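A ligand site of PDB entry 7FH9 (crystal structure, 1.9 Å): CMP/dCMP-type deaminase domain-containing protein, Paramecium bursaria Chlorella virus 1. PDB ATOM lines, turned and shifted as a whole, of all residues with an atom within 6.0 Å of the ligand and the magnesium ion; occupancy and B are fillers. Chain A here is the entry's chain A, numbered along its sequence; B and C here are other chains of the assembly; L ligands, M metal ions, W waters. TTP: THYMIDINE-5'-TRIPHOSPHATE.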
ATOM      1  N   PHE A  18      -8.923  -8.957   4.345  1.00  0.00           N
ATOM      2  CA  PHE A  18      -9.331  -7.696   3.725  1.00  0.00           C
ATOM      3  C   PHE A  18      -9.966  -7.831   2.351  1.00  0.00           C
ATOM      4  O   PHE A  18     -10.779  -6.982   1.989  1.00  0.00           O
ATOM      5  CB  PHE A  18      -8.137  -6.740   3.627  1.00  0.00           C
ATOM      6  CG  PHE A  18      -7.731  -6.147   4.941  1.00  0.00           C
ATOM      7  CD1 PHE A  18      -8.409  -5.049   5.457  1.00  0.00           C
ATOM      8  CD2 PHE A  18      -6.691  -6.684   5.674  1.00  0.00           C
ATOM      9  CE1 PHE A  18      -8.048  -4.511   6.666  1.00  0.00           C
ATOM     10  CE2 PHE A  18      -6.335  -6.140   6.895  1.00  0.00           C
ATOM     11  CZ  PHE A  18      -7.011  -5.049   7.390  1.00  0.00           C
ATOM     12  N   LYS A  20     -12.431  -8.536  -0.540  1.00  0.00           N
ATOM     13  CA  LYS A  20     -13.863  -8.813  -0.623  1.00  0.00           C
ATOM     14  C   LYS A  20     -14.224  -9.725  -1.792  1.00  0.00           C
ATOM     15  O   LYS A  20     -15.405 -10.051  -1.965  1.00  0.00           O
ATOM     16  CB  LYS A  20     -14.658  -7.512  -0.724  1.00  0.00           C
ATOM     17  CG  LYS A  20     -14.459  -6.552   0.440  1.00  0.00           C
ATOM     18  CD  LYS A  20     -15.611  -5.567   0.536  1.00  0.00           C
ATOM     19  CE  LYS A  20     -15.360  -4.487   1.570  1.00  0.00           C
ATOM     20  NZ  LYS A  20     -14.377  -3.485   1.068  1.00  0.00           N
ATOM     21  N   VAL A  40       1.033  -2.178   1.110  1.00  0.00           N
ATOM     22  CA  VAL A  40       0.218  -3.387   0.998  1.00  0.00           C
ATOM     23  C   VAL A  40      -0.800  -3.194  -0.110  1.00  0.00           C
ATOM     24  O   VAL A  40      -1.414  -2.137  -0.228  1.00  0.00           O
ATOM     25  CB  VAL A  40      -0.497  -3.725   2.330  1.00  0.00           C
ATOM     26  CG1 VAL A  40      -1.437  -4.911   2.140  1.00  0.00           C
ATOM     27  CG2 VAL A  40       0.522  -4.000   3.428  1.00  0.00           C
ATOM     28  N   GLY A  41      -0.962  -4.232  -0.936  1.00  0.00           N
ATOM     29  CA  GLY A  41      -2.040  -4.267  -1.907  1.00  0.00           C
ATOM     30  C   GLY A  41      -2.869  -5.528  -1.709  1.00  0.00           C
ATOM     31  O   GLY A  41      -2.365  -6.572  -1.290  1.00  0.00           O
ATOM     32  N   TYR A  42      -4.158  -5.415  -2.023  1.00  0.00           N
ATOM     33  CA  TYR A  42      -5.007  -6.598  -2.138  1.00  0.00           C
ATOM     34  C   TYR A  42      -6.031  -6.316  -3.224  1.00  0.00           C
ATOM     35  O   TYR A  42      -6.280  -5.159  -3.564  1.00  0.00           O
ATOM     36  CB  TYR A  42      -5.651  -6.986  -0.791  1.00  0.00           C
ATOM     37  CG  TYR A  42      -6.402  -5.887  -0.069  1.00  0.00           C
ATOM     38  CD1 TYR A  42      -5.747  -5.056   0.841  1.00  0.00           C
ATOM     39  CD2 TYR A  42      -7.768  -5.693  -0.262  1.00  0.00           C
ATOM     40  CE1 TYR A  42      -6.429  -4.054   1.531  1.00  0.00           C
ATOM     41  CE2 TYR A  42      -8.470  -4.683   0.424  1.00  0.00           C
ATOM     42  CZ  TYR A  42      -7.780  -3.863   1.313  1.00  0.00           C
ATOM     43  OH  TYR A  42      -8.429  -2.864   2.003  1.00  0.00           O
ATOM     44  N   ASN A  43      -6.570  -7.377  -3.812  1.00  0.00           N
ATOM     45  CA  ASN A  43      -7.487  -7.164  -4.925  1.00  0.00           C
ATOM     46  C   ASN A  43      -8.802  -6.588  -4.420  1.00  0.00           C
ATOM     47  O   ASN A  43      -9.290  -6.957  -3.352  1.00  0.00           O
ATOM     48  CB  ASN A  43      -7.720  -8.459  -5.733  1.00  0.00           C
ATOM     49  CG  ASN A  43      -8.238  -9.629  -4.898  1.00  0.00           C
ATOM     50  OD1 ASN A  43      -7.905  -9.790  -3.722  1.00  0.00           O
ATOM     51  ND2 ASN A  43      -9.058 -10.474  -5.526  1.00  0.00           N
ATOM     52  N   GLY A  44      -9.346  -5.631  -5.165  1.00  0.00           N
ATOM     53  CA  GLY A  44     -10.538  -4.953  -4.705  1.00  0.00           C
ATOM     54  C   GLY A  44     -11.017  -3.948  -5.734  1.00  0.00           C
ATOM     55  O   GLY A  44     -10.393  -3.734  -6.773  1.00  0.00           O
ATOM     56  N   LEU A  45     -12.154  -3.321  -5.403  1.00  0.00           N
ATOM     57  CA  LEU A  45     -12.683  -2.278  -6.261  1.00  0.00           C
ATOM     58  C   LEU A  45     -12.082  -0.944  -5.848  1.00  0.00           C
ATOM     59  O   LEU A  45     -11.511  -0.829  -4.759  1.00  0.00           O
ATOM     60  CB  LEU A  45     -14.224  -2.253  -6.168  1.00  0.00           C
ATOM     61  CG  LEU A  45     -14.961  -3.586  -6.396  1.00  0.00           C
ATOM     62  CD1 LEU A  45     -16.466  -3.338  -6.612  1.00  0.00           C
ATOM     63  CD2 LEU A  45     -14.367  -4.411  -7.549  1.00  0.00           C
ATOM     64  N   PRO A  46     -12.160   0.092  -6.698  1.00  0.00           N
ATOM     65  CA  PRO A  46     -11.550   1.369  -6.313  1.00  0.00           C
ATOM     66  C   PRO A  46     -12.136   1.922  -5.029  1.00  0.00           C
ATOM     67  O   PRO A  46     -13.302   1.700  -4.700  1.00  0.00           O
ATOM     68  CB  PRO A  46     -11.866   2.278  -7.501  1.00  0.00           C
ATOM     69  CG  PRO A  46     -12.027   1.309  -8.677  1.00  0.00           C
ATOM     70  CD  PRO A  46     -12.771   0.161  -8.034  1.00  0.00           C
ATOM     71  N   ARG A  47     -11.285   2.631  -4.276  1.00  0.00           N
ATOM     72  CA  ARG A  47     -11.657   3.221  -2.963  1.00  0.00           C
ATOM     73  C   ARG A  47     -12.926   4.078  -3.098  1.00  0.00           C
ATOM     74  O   ARG A  47     -12.923   5.016  -3.930  1.00  0.00           O
ATOM     75  CB  ARG A  47     -10.493   4.050  -2.406  1.00  0.00           C
ATOM     76  CG  ARG A  47     -10.857   4.875  -1.172  1.00  0.00           C
ATOM     77  CD  ARG A  47      -9.749   5.839  -0.784  1.00  0.00           C
ATOM     78  NE  ARG A  47      -9.549   6.895  -1.763  1.00  0.00           N
ATOM     79  CZ  ARG A  47      -8.619   6.873  -2.714  1.00  0.00           C
ATOM     80  NH1 ARG A  47      -7.797   5.840  -2.819  1.00  0.00           N
ATOM     81  NH2 ARG A  47      -8.528   7.878  -3.564  1.00  0.00           N
ATOM     82  N   GLY A  48     -13.949   3.765  -2.315  1.00  0.00           N
ATOM     83  CA  GLY A  48     -15.193   4.506  -2.303  1.00  0.00           C
ATOM     84  C   GLY A  48     -16.216   4.077  -3.336  1.00  0.00           C
ATOM     85  O   GLY A  48     -17.357   4.556  -3.291  1.00  0.00           O
ATOM     86  N   PHE A  49     -15.862   3.188  -4.260  1.00  0.00           N
ATOM     87  CA  PHE A  49     -16.816   2.686  -5.242  1.00  0.00           C
ATOM     88  C   PHE A  49     -17.770   1.729  -4.543  1.00  0.00           C
ATOM     89  O   PHE A  49     -17.336   0.853  -3.803  1.00  0.00           O
ATOM     90  CB  PHE A  49     -16.065   1.947  -6.364  1.00  0.00           C
ATOM     91  CG  PHE A  49     -16.851   1.784  -7.640  1.00  0.00           C
ATOM     92  CD1 PHE A  49     -17.329   2.900  -8.323  1.00  0.00           C
ATOM     93  CD2 PHE A  49     -17.075   0.519  -8.169  1.00  0.00           C
ATOM     94  CE1 PHE A  49     -18.022   2.756  -9.505  1.00  0.00           C
ATOM     95  CE2 PHE A  49     -17.763   0.362  -9.351  1.00  0.00           C
ATOM     96  CZ  PHE A  49     -18.247   1.484 -10.022  1.00  0.00           C
ATOM     97  N   GLU A  51     -19.643  -1.214  -3.431  1.00  0.00           N
ATOM     98  CA  GLU A  51     -19.289  -2.608  -3.669  1.00  0.00           C
ATOM     99  C   GLU A  51     -20.533  -3.491  -3.595  1.00  0.00           C
ATOM    100  O   GLU A  51     -20.732  -4.278  -2.665  1.00  0.00           O
ATOM    101  CB  GLU A  51     -18.224  -3.049  -2.681  1.00  0.00           C
ATOM    102  CG  GLU A  51     -16.992  -2.170  -2.750  1.00  0.00           C
ATOM    103  CD  GLU A  51     -15.779  -2.813  -2.115  1.00  0.00           C
ATOM    104  OE1 GLU A  51     -15.426  -3.925  -2.519  1.00  0.00           O
ATOM    105  OE2 GLU A  51     -15.201  -2.174  -1.206  1.00  0.00           O
ATOM    106  N   VAL A  66      -9.126  -4.160  -9.231  1.00  0.00           N
ATOM    107  CA  VAL A  66      -7.701  -3.835  -9.311  1.00  0.00           C
ATOM    108  C   VAL A  66      -6.926  -5.015  -8.741  1.00  0.00           C
ATOM    109  O   VAL A  66      -7.267  -5.511  -7.653  1.00  0.00           O
ATOM    110  CB  VAL A  66      -7.365  -2.550  -8.536  1.00  0.00           C
ATOM    111  CG1 VAL A  66      -5.833  -2.248  -8.606  1.00  0.00           C
ATOM    112  CG2 VAL A  66      -8.195  -1.351  -9.047  1.00  0.00           C
ATOM    113  N   ALA A  68      -3.947  -7.085  -6.859  1.00  0.00           N
ATOM    114  CA  ALA A  68      -3.272  -6.774  -5.597  1.00  0.00           C
ATOM    115  C   ALA A  68      -1.927  -6.083  -5.828  1.00  0.00           C
ATOM    116  O   ALA A  68      -1.576  -5.137  -5.107  1.00  0.00           O
ATOM    117  CB  ALA A  68      -3.069  -8.059  -4.787  1.00  0.00           C
ATOM    118  N   ASN A  71      -2.356  -2.621  -7.018  1.00  0.00           N
ATOM    119  CA  ASN A  71      -2.842  -1.812  -5.910  1.00  0.00           C
ATOM    120  C   ASN A  71      -1.725  -1.433  -4.946  1.00  0.00           C
ATOM    121  O   ASN A  71      -1.720  -0.320  -4.418  1.00  0.00           O
ATOM    122  CB  ASN A  71      -3.948  -2.544  -5.137  1.00  0.00           C
ATOM    123  CG  ASN A  71      -5.296  -1.864  -5.264  1.00  0.00           C
ATOM    124  OD1 ASN A  71      -5.369  -0.650  -5.490  1.00  0.00           O
ATOM    125  ND2 ASN A  71      -6.366  -2.624  -5.084  1.00  0.00           N
ATOM    126  N   ALA A  72      -0.793  -2.354  -4.688  1.00  0.00           N
ATOM    127  CA  ALA A  72       0.308  -2.042  -3.784  1.00  0.00           C
ATOM    128  C   ALA A  72       1.127  -0.874  -4.317  1.00  0.00           C
ATOM    129  O   ALA A  72       1.597  -0.013  -3.550  1.00  0.00           O
ATOM    130  CB  ALA A  72       1.206  -3.260  -3.591  1.00  0.00           C
ATOM    131  N   THR A  75      -1.058   2.378  -4.330  1.00  0.00           N
ATOM    132  CA  THR A  75      -1.207   2.853  -2.950  1.00  0.00           C
ATOM    133  C   THR A  75       0.074   3.549  -2.478  1.00  0.00           C
ATOM    134  O   THR A  75       0.008   4.558  -1.753  1.00  0.00           O
ATOM    135  CB  THR A  75      -1.566   1.665  -2.049  1.00  0.00           C
ATOM    136  OG1 THR A  75      -2.839   1.145  -2.451  1.00  0.00           O
ATOM    137  CG2 THR A  75      -1.630   2.096  -0.574  1.00  0.00           C
ATOM    138  N   GLN B 104      -6.903   4.983  -7.391  1.00  0.00           N
ATOM    139  CA  GLN B 104      -6.159   4.363  -6.302  1.00  0.00           C
ATOM    140  C   GLN B 104      -4.973   5.206  -5.861  1.00  0.00           C
ATOM    141  O   GLN B 104      -4.587   5.168  -4.687  1.00  0.00           O
ATOM    142  CB  GLN B 104      -5.701   2.958  -6.691  1.00  0.00           C
ATOM    143  CG  GLN B 104      -6.853   1.941  -6.704  1.00  0.00           C
ATOM    144  CD  GLN B 104      -7.586   1.926  -5.379  1.00  0.00           C
ATOM    145  OE1 GLN B 104      -7.164   1.252  -4.429  1.00  0.00           O
ATOM    146  NE2 GLN B 104      -8.661   2.690  -5.300  1.00  0.00           N
ATOM    147  N   LYS C   3     -12.463  -3.134  10.678  1.00  0.00           N
ATOM    148  CA  LYS C   3     -11.080  -3.011  10.224  1.00  0.00           C
ATOM    149  C   LYS C   3     -10.098  -2.946  11.384  1.00  0.00           C
ATOM    150  O   LYS C   3      -9.006  -3.517  11.295  1.00  0.00           O
ATOM    151  CB  LYS C   3     -10.906  -1.798   9.318  1.00  0.00           C
ATOM    152  CG  LYS C   3     -11.568  -1.987   7.950  1.00  0.00           C
ATOM    153  CD  LYS C   3     -11.095  -0.987   6.929  1.00  0.00           C
ATOM    154  CE  LYS C   3     -11.701  -1.306   5.549  1.00  0.00           C
ATOM    155  NZ  LYS C   3     -12.044  -0.084   4.774  1.00  0.00           N
ATOM    156  N   ASN C  34      -5.215   6.669   6.264  1.00  0.00           N
ATOM    157  CA  ASN C  34      -5.585   5.963   5.049  1.00  0.00           C
ATOM    158  C   ASN C  34      -5.500   4.453   5.206  1.00  0.00           C
ATOM    159  O   ASN C  34      -5.550   3.735   4.213  1.00  0.00           O
ATOM    160  CB  ASN C  34      -4.714   6.426   3.881  1.00  0.00           C
ATOM    161  CG  ASN C  34      -5.053   7.828   3.421  1.00  0.00           C
ATOM    162  OD1 ASN C  34      -6.146   8.334   3.680  1.00  0.00           O
ATOM    163  ND2 ASN C  34      -4.136   8.465   2.694  1.00  0.00           N
ATOM    164  N   ASN C  35      -5.376   3.972   6.443  1.00  0.00           N
ATOM    165  CA  ASN C  35      -5.280   2.558   6.795  1.00  0.00           C
ATOM    166  C   ASN C  35      -4.010   1.898   6.243  1.00  0.00           C
ATOM    167  O   ASN C  35      -3.956   0.685   6.049  1.00  0.00           O
ATOM    168  CB  ASN C  35      -6.549   1.799   6.360  1.00  0.00           C
ATOM    169  CG  ASN C  35      -7.745   2.146   7.239  1.00  0.00           C
ATOM    170  OD1 ASN C  35      -7.577   2.511   8.410  1.00  0.00           O
ATOM    171  ND2 ASN C  35      -8.945   2.016   6.695  1.00  0.00           N
ATOM    172  N   ASN C  36      -2.963   2.695   6.034  1.00  0.00           N
ATOM    173  CA  ASN C  36      -1.635   2.187   5.665  1.00  0.00           C
ATOM    174  C   ASN C  36      -0.864   1.858   6.939  1.00  0.00           C
ATOM    175  O   ASN C  36      -0.958   2.562   7.939  1.00  0.00           O
ATOM    176  CB  ASN C  36      -0.892   3.218   4.814  1.00  0.00           C
ATOM    177  CG  ASN C  36       0.538   2.805   4.461  1.00  0.00           C
ATOM    178  OD1 ASN C  36       0.759   1.915   3.645  1.00  0.00           O
ATOM    179  ND2 ASN C  36       1.520   3.489   5.057  1.00  0.00           N
HETATM  180  PA  TTP L   1     -11.407  -1.226   0.626  1.00  0.00           P
HETATM  181  O1A TTP L   1     -11.112  -2.281   1.629  1.00  0.00           O
HETATM  182  O2A TTP L   1     -12.503  -1.463  -0.365  1.00  0.00           O
HETATM  183  O3A TTP L   1     -11.698   0.155   1.388  1.00  0.00           O
HETATM  184  PB  TTP L   1     -12.599   1.429   1.029  1.00  0.00           P
HETATM  185  O1B TTP L   1     -11.809   2.662   1.306  1.00  0.00           O
HETATM  186  O2B TTP L   1     -13.199   1.217  -0.325  1.00  0.00           O
HETATM  187  O3B TTP L   1     -13.753   1.300   2.130  1.00  0.00           O
HETATM  188  PG  TTP L   1     -14.961   0.245   2.332  1.00  0.00           P
HETATM  189  O1G TTP L   1     -15.157  -0.418   0.987  1.00  0.00           O
HETATM  190  O2G TTP L   1     -14.490  -0.725   3.391  1.00  0.00           O
HETATM  191  O3G TTP L   1     -16.161   1.054   2.766  1.00  0.00           O
HETATM  192  O5' TTP L   1     -10.066  -0.854  -0.166  1.00  0.00           O
HETATM  193  C5' TTP L   1     -10.111   0.176  -1.186  1.00  0.00           C
HETATM  194  C4' TTP L   1      -9.285  -0.254  -2.376  1.00  0.00           C
HETATM  195  O4' TTP L   1      -7.901   0.077  -2.145  1.00  0.00           O
HETATM  196  C3' TTP L   1      -9.324  -1.749  -2.669  1.00  0.00           C
HETATM  197  O3' TTP L   1      -9.205  -1.988  -4.061  1.00  0.00           O
HETATM  198  C2' TTP L   1      -8.097  -2.265  -1.928  1.00  0.00           C
HETATM  199  C1' TTP L   1      -7.122  -1.110  -2.065  1.00  0.00           C
HETATM  200  N1  TTP L   1      -6.186  -0.964  -0.933  1.00  0.00           N
HETATM  201  C2  TTP L   1      -4.904  -1.455  -1.077  1.00  0.00           C
HETATM  202  O2  TTP L   1      -4.511  -2.003  -2.093  1.00  0.00           O
HETATM  203  N3  TTP L   1      -4.098  -1.273   0.020  1.00  0.00           N
HETATM  204  C4  TTP L   1      -4.435  -0.665   1.212  1.00  0.00           C
HETATM  205  O4  TTP L   1      -3.603  -0.582   2.122  1.00  0.00           O
HETATM  206  C5  TTP L   1      -5.794  -0.180   1.297  1.00  0.00           C
HETATM  207  C5M TTP L   1      -6.240   0.497   2.558  1.00  0.00           C
HETATM  208  C6  TTP L   1      -6.595  -0.345   0.228  1.00  0.00           C
HETATM  209 MG    MG M   1     -14.263  -0.341  -0.816  1.00  0.00          MG
HETATM  210  O   HOH W   1     -17.611  -1.654   0.828  1.00  0.00           O
HETATM  211  O   HOH W   2      -9.073   2.139   1.931  1.00  0.00           O
HETATM  212  O   HOH W   3      -3.158  -1.501   4.811  1.00  0.00           O
HETATM  213  O   HOH W   4     -15.785   0.955  -1.670  1.00  0.00           O
HETATM  214  O   HOH W   5     -13.580  -0.243  -2.796  1.00  0.00           O
HETATM  215  O   HOH W   6     -12.710  -3.611  -2.439  1.00  0.00           O
HETATM  216  O   HOH W   7      -0.604   0.089   2.345  1.00  0.00           O
HETATM  217  O   HOH W   8     -17.469   2.187   0.030  1.00  0.00           O
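Lys 20 touches the magnesium ion. Two residues have an atom within 4 Å of the magnesium ion: Lys 20 and Glu 51. The nearest printed residue that does not touch the magnesium ion is Gly 48 (4.4 Å).
NZ of Lys 20 is in salt-bridge range of OE1 of Glu 51, at 3.8 Å. The side-chain amide oxygen of Asn 71 lies close to the side-chain amide oxygen of Gln 104 of chain B, at 2.8 Å. The side-chain amide nitrogen (NE2) of Gln 104 of chain B lies close to the backbone NH (N) of Arg 47 (2.8 Å). The side-chain amide nitrogen of Asn 71 sits at hydrogen-bond distance from the backbone carbonyl oxygen of Tyr 42 (3.0 Å). The side-chain hydroxyl (OG1) of Thr 75 lies within hydrogen-bond range of the backbone carbonyl oxygen (O) of Asn 71. O of Gly 44 is in hydrogen-bond range of N of Val 66 (2.8 Å).
OE1 of Gln 104 of chain B sits close to O4' of the ligand (2.7 Å). The backbone carbonyl oxygen (O) of Leu 45 is in hydrogen-bond range of an oxygen (O3') of the ligand (2.7 Å). N of Tyr 42 is in hydrogen-bond range of O2 of the ligand, 3.4 Å away. OH of Tyr 42 is in hydrogen-bond range of O1A of the ligand, 2.8 Å away. The backbone carbonyl oxygen (O) of Val 40 is in hydrogen-bond range of a nitrogen (N3) of the ligand, 2.8 Å away. The side-chain amino group (NZ) of Lys 3 of chain C is in salt-bridge range of an oxygen (O2G) of the ligand (2.9 Å). ND2 of Asn 71 is in hydrogen-bond range of O3' of the ligand (3.1 Å). NZ of Lys 20 lies within salt-bridge range of O1A of the ligand, 3.5 Å away. The backbone carbonyl oxygen of Gly 44 sits close to an oxygen (O3') of the ligand (3.4 Å). N of Gly 48 sits close to O2B of the ligand (3.3 Å).
Water W3 lies within hydrogen-bond range of O of Asn 35 of chain C (2.6 Å) and O4 of the ligand (2.9 Å). Water W6 lies within hydrogen-bond range of the side-chain carboxylate of Glu 51 (2.7 Å) and the backbone NH of Leu 45 (3.0 Å). Water W7 lies within hydrogen-bond range of OD1 of Asn 36 of chain C, N of Val 40 and O4 of the ligand.
Residues that only touch the ligand: Gly 41 (3.4 Å), Arg 47 (3.5 Å), Thr 75 (3.6 Å) and Asn 34 of chain C (3.7 Å). Hydrophobic or aromatic side chains that line the ligand: Tyr 42. 14 residues have an atom within 4 Å of the ligand: Lys 20, Val 40, Gly 41, Tyr 42, Gly 44, Leu 45, Arg 47, Gly 48, Glu 51, Asn 71, Thr 75, Gln 104 of chain B, Lys 3 of chain C and Asn 34 of chain C. Along chain A the residues within 4 Å of the ligand span positions 20 to 75.
The magnesium ion is bound by O2B of the ligand (1.9 Å), O1G of the ligand (2.0 Å), OE2 of Glu 51 (2.1 Å), water W5 (2.1 Å), O2A of the ligand (2.1 Å) and water W4 (2.2 Å).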
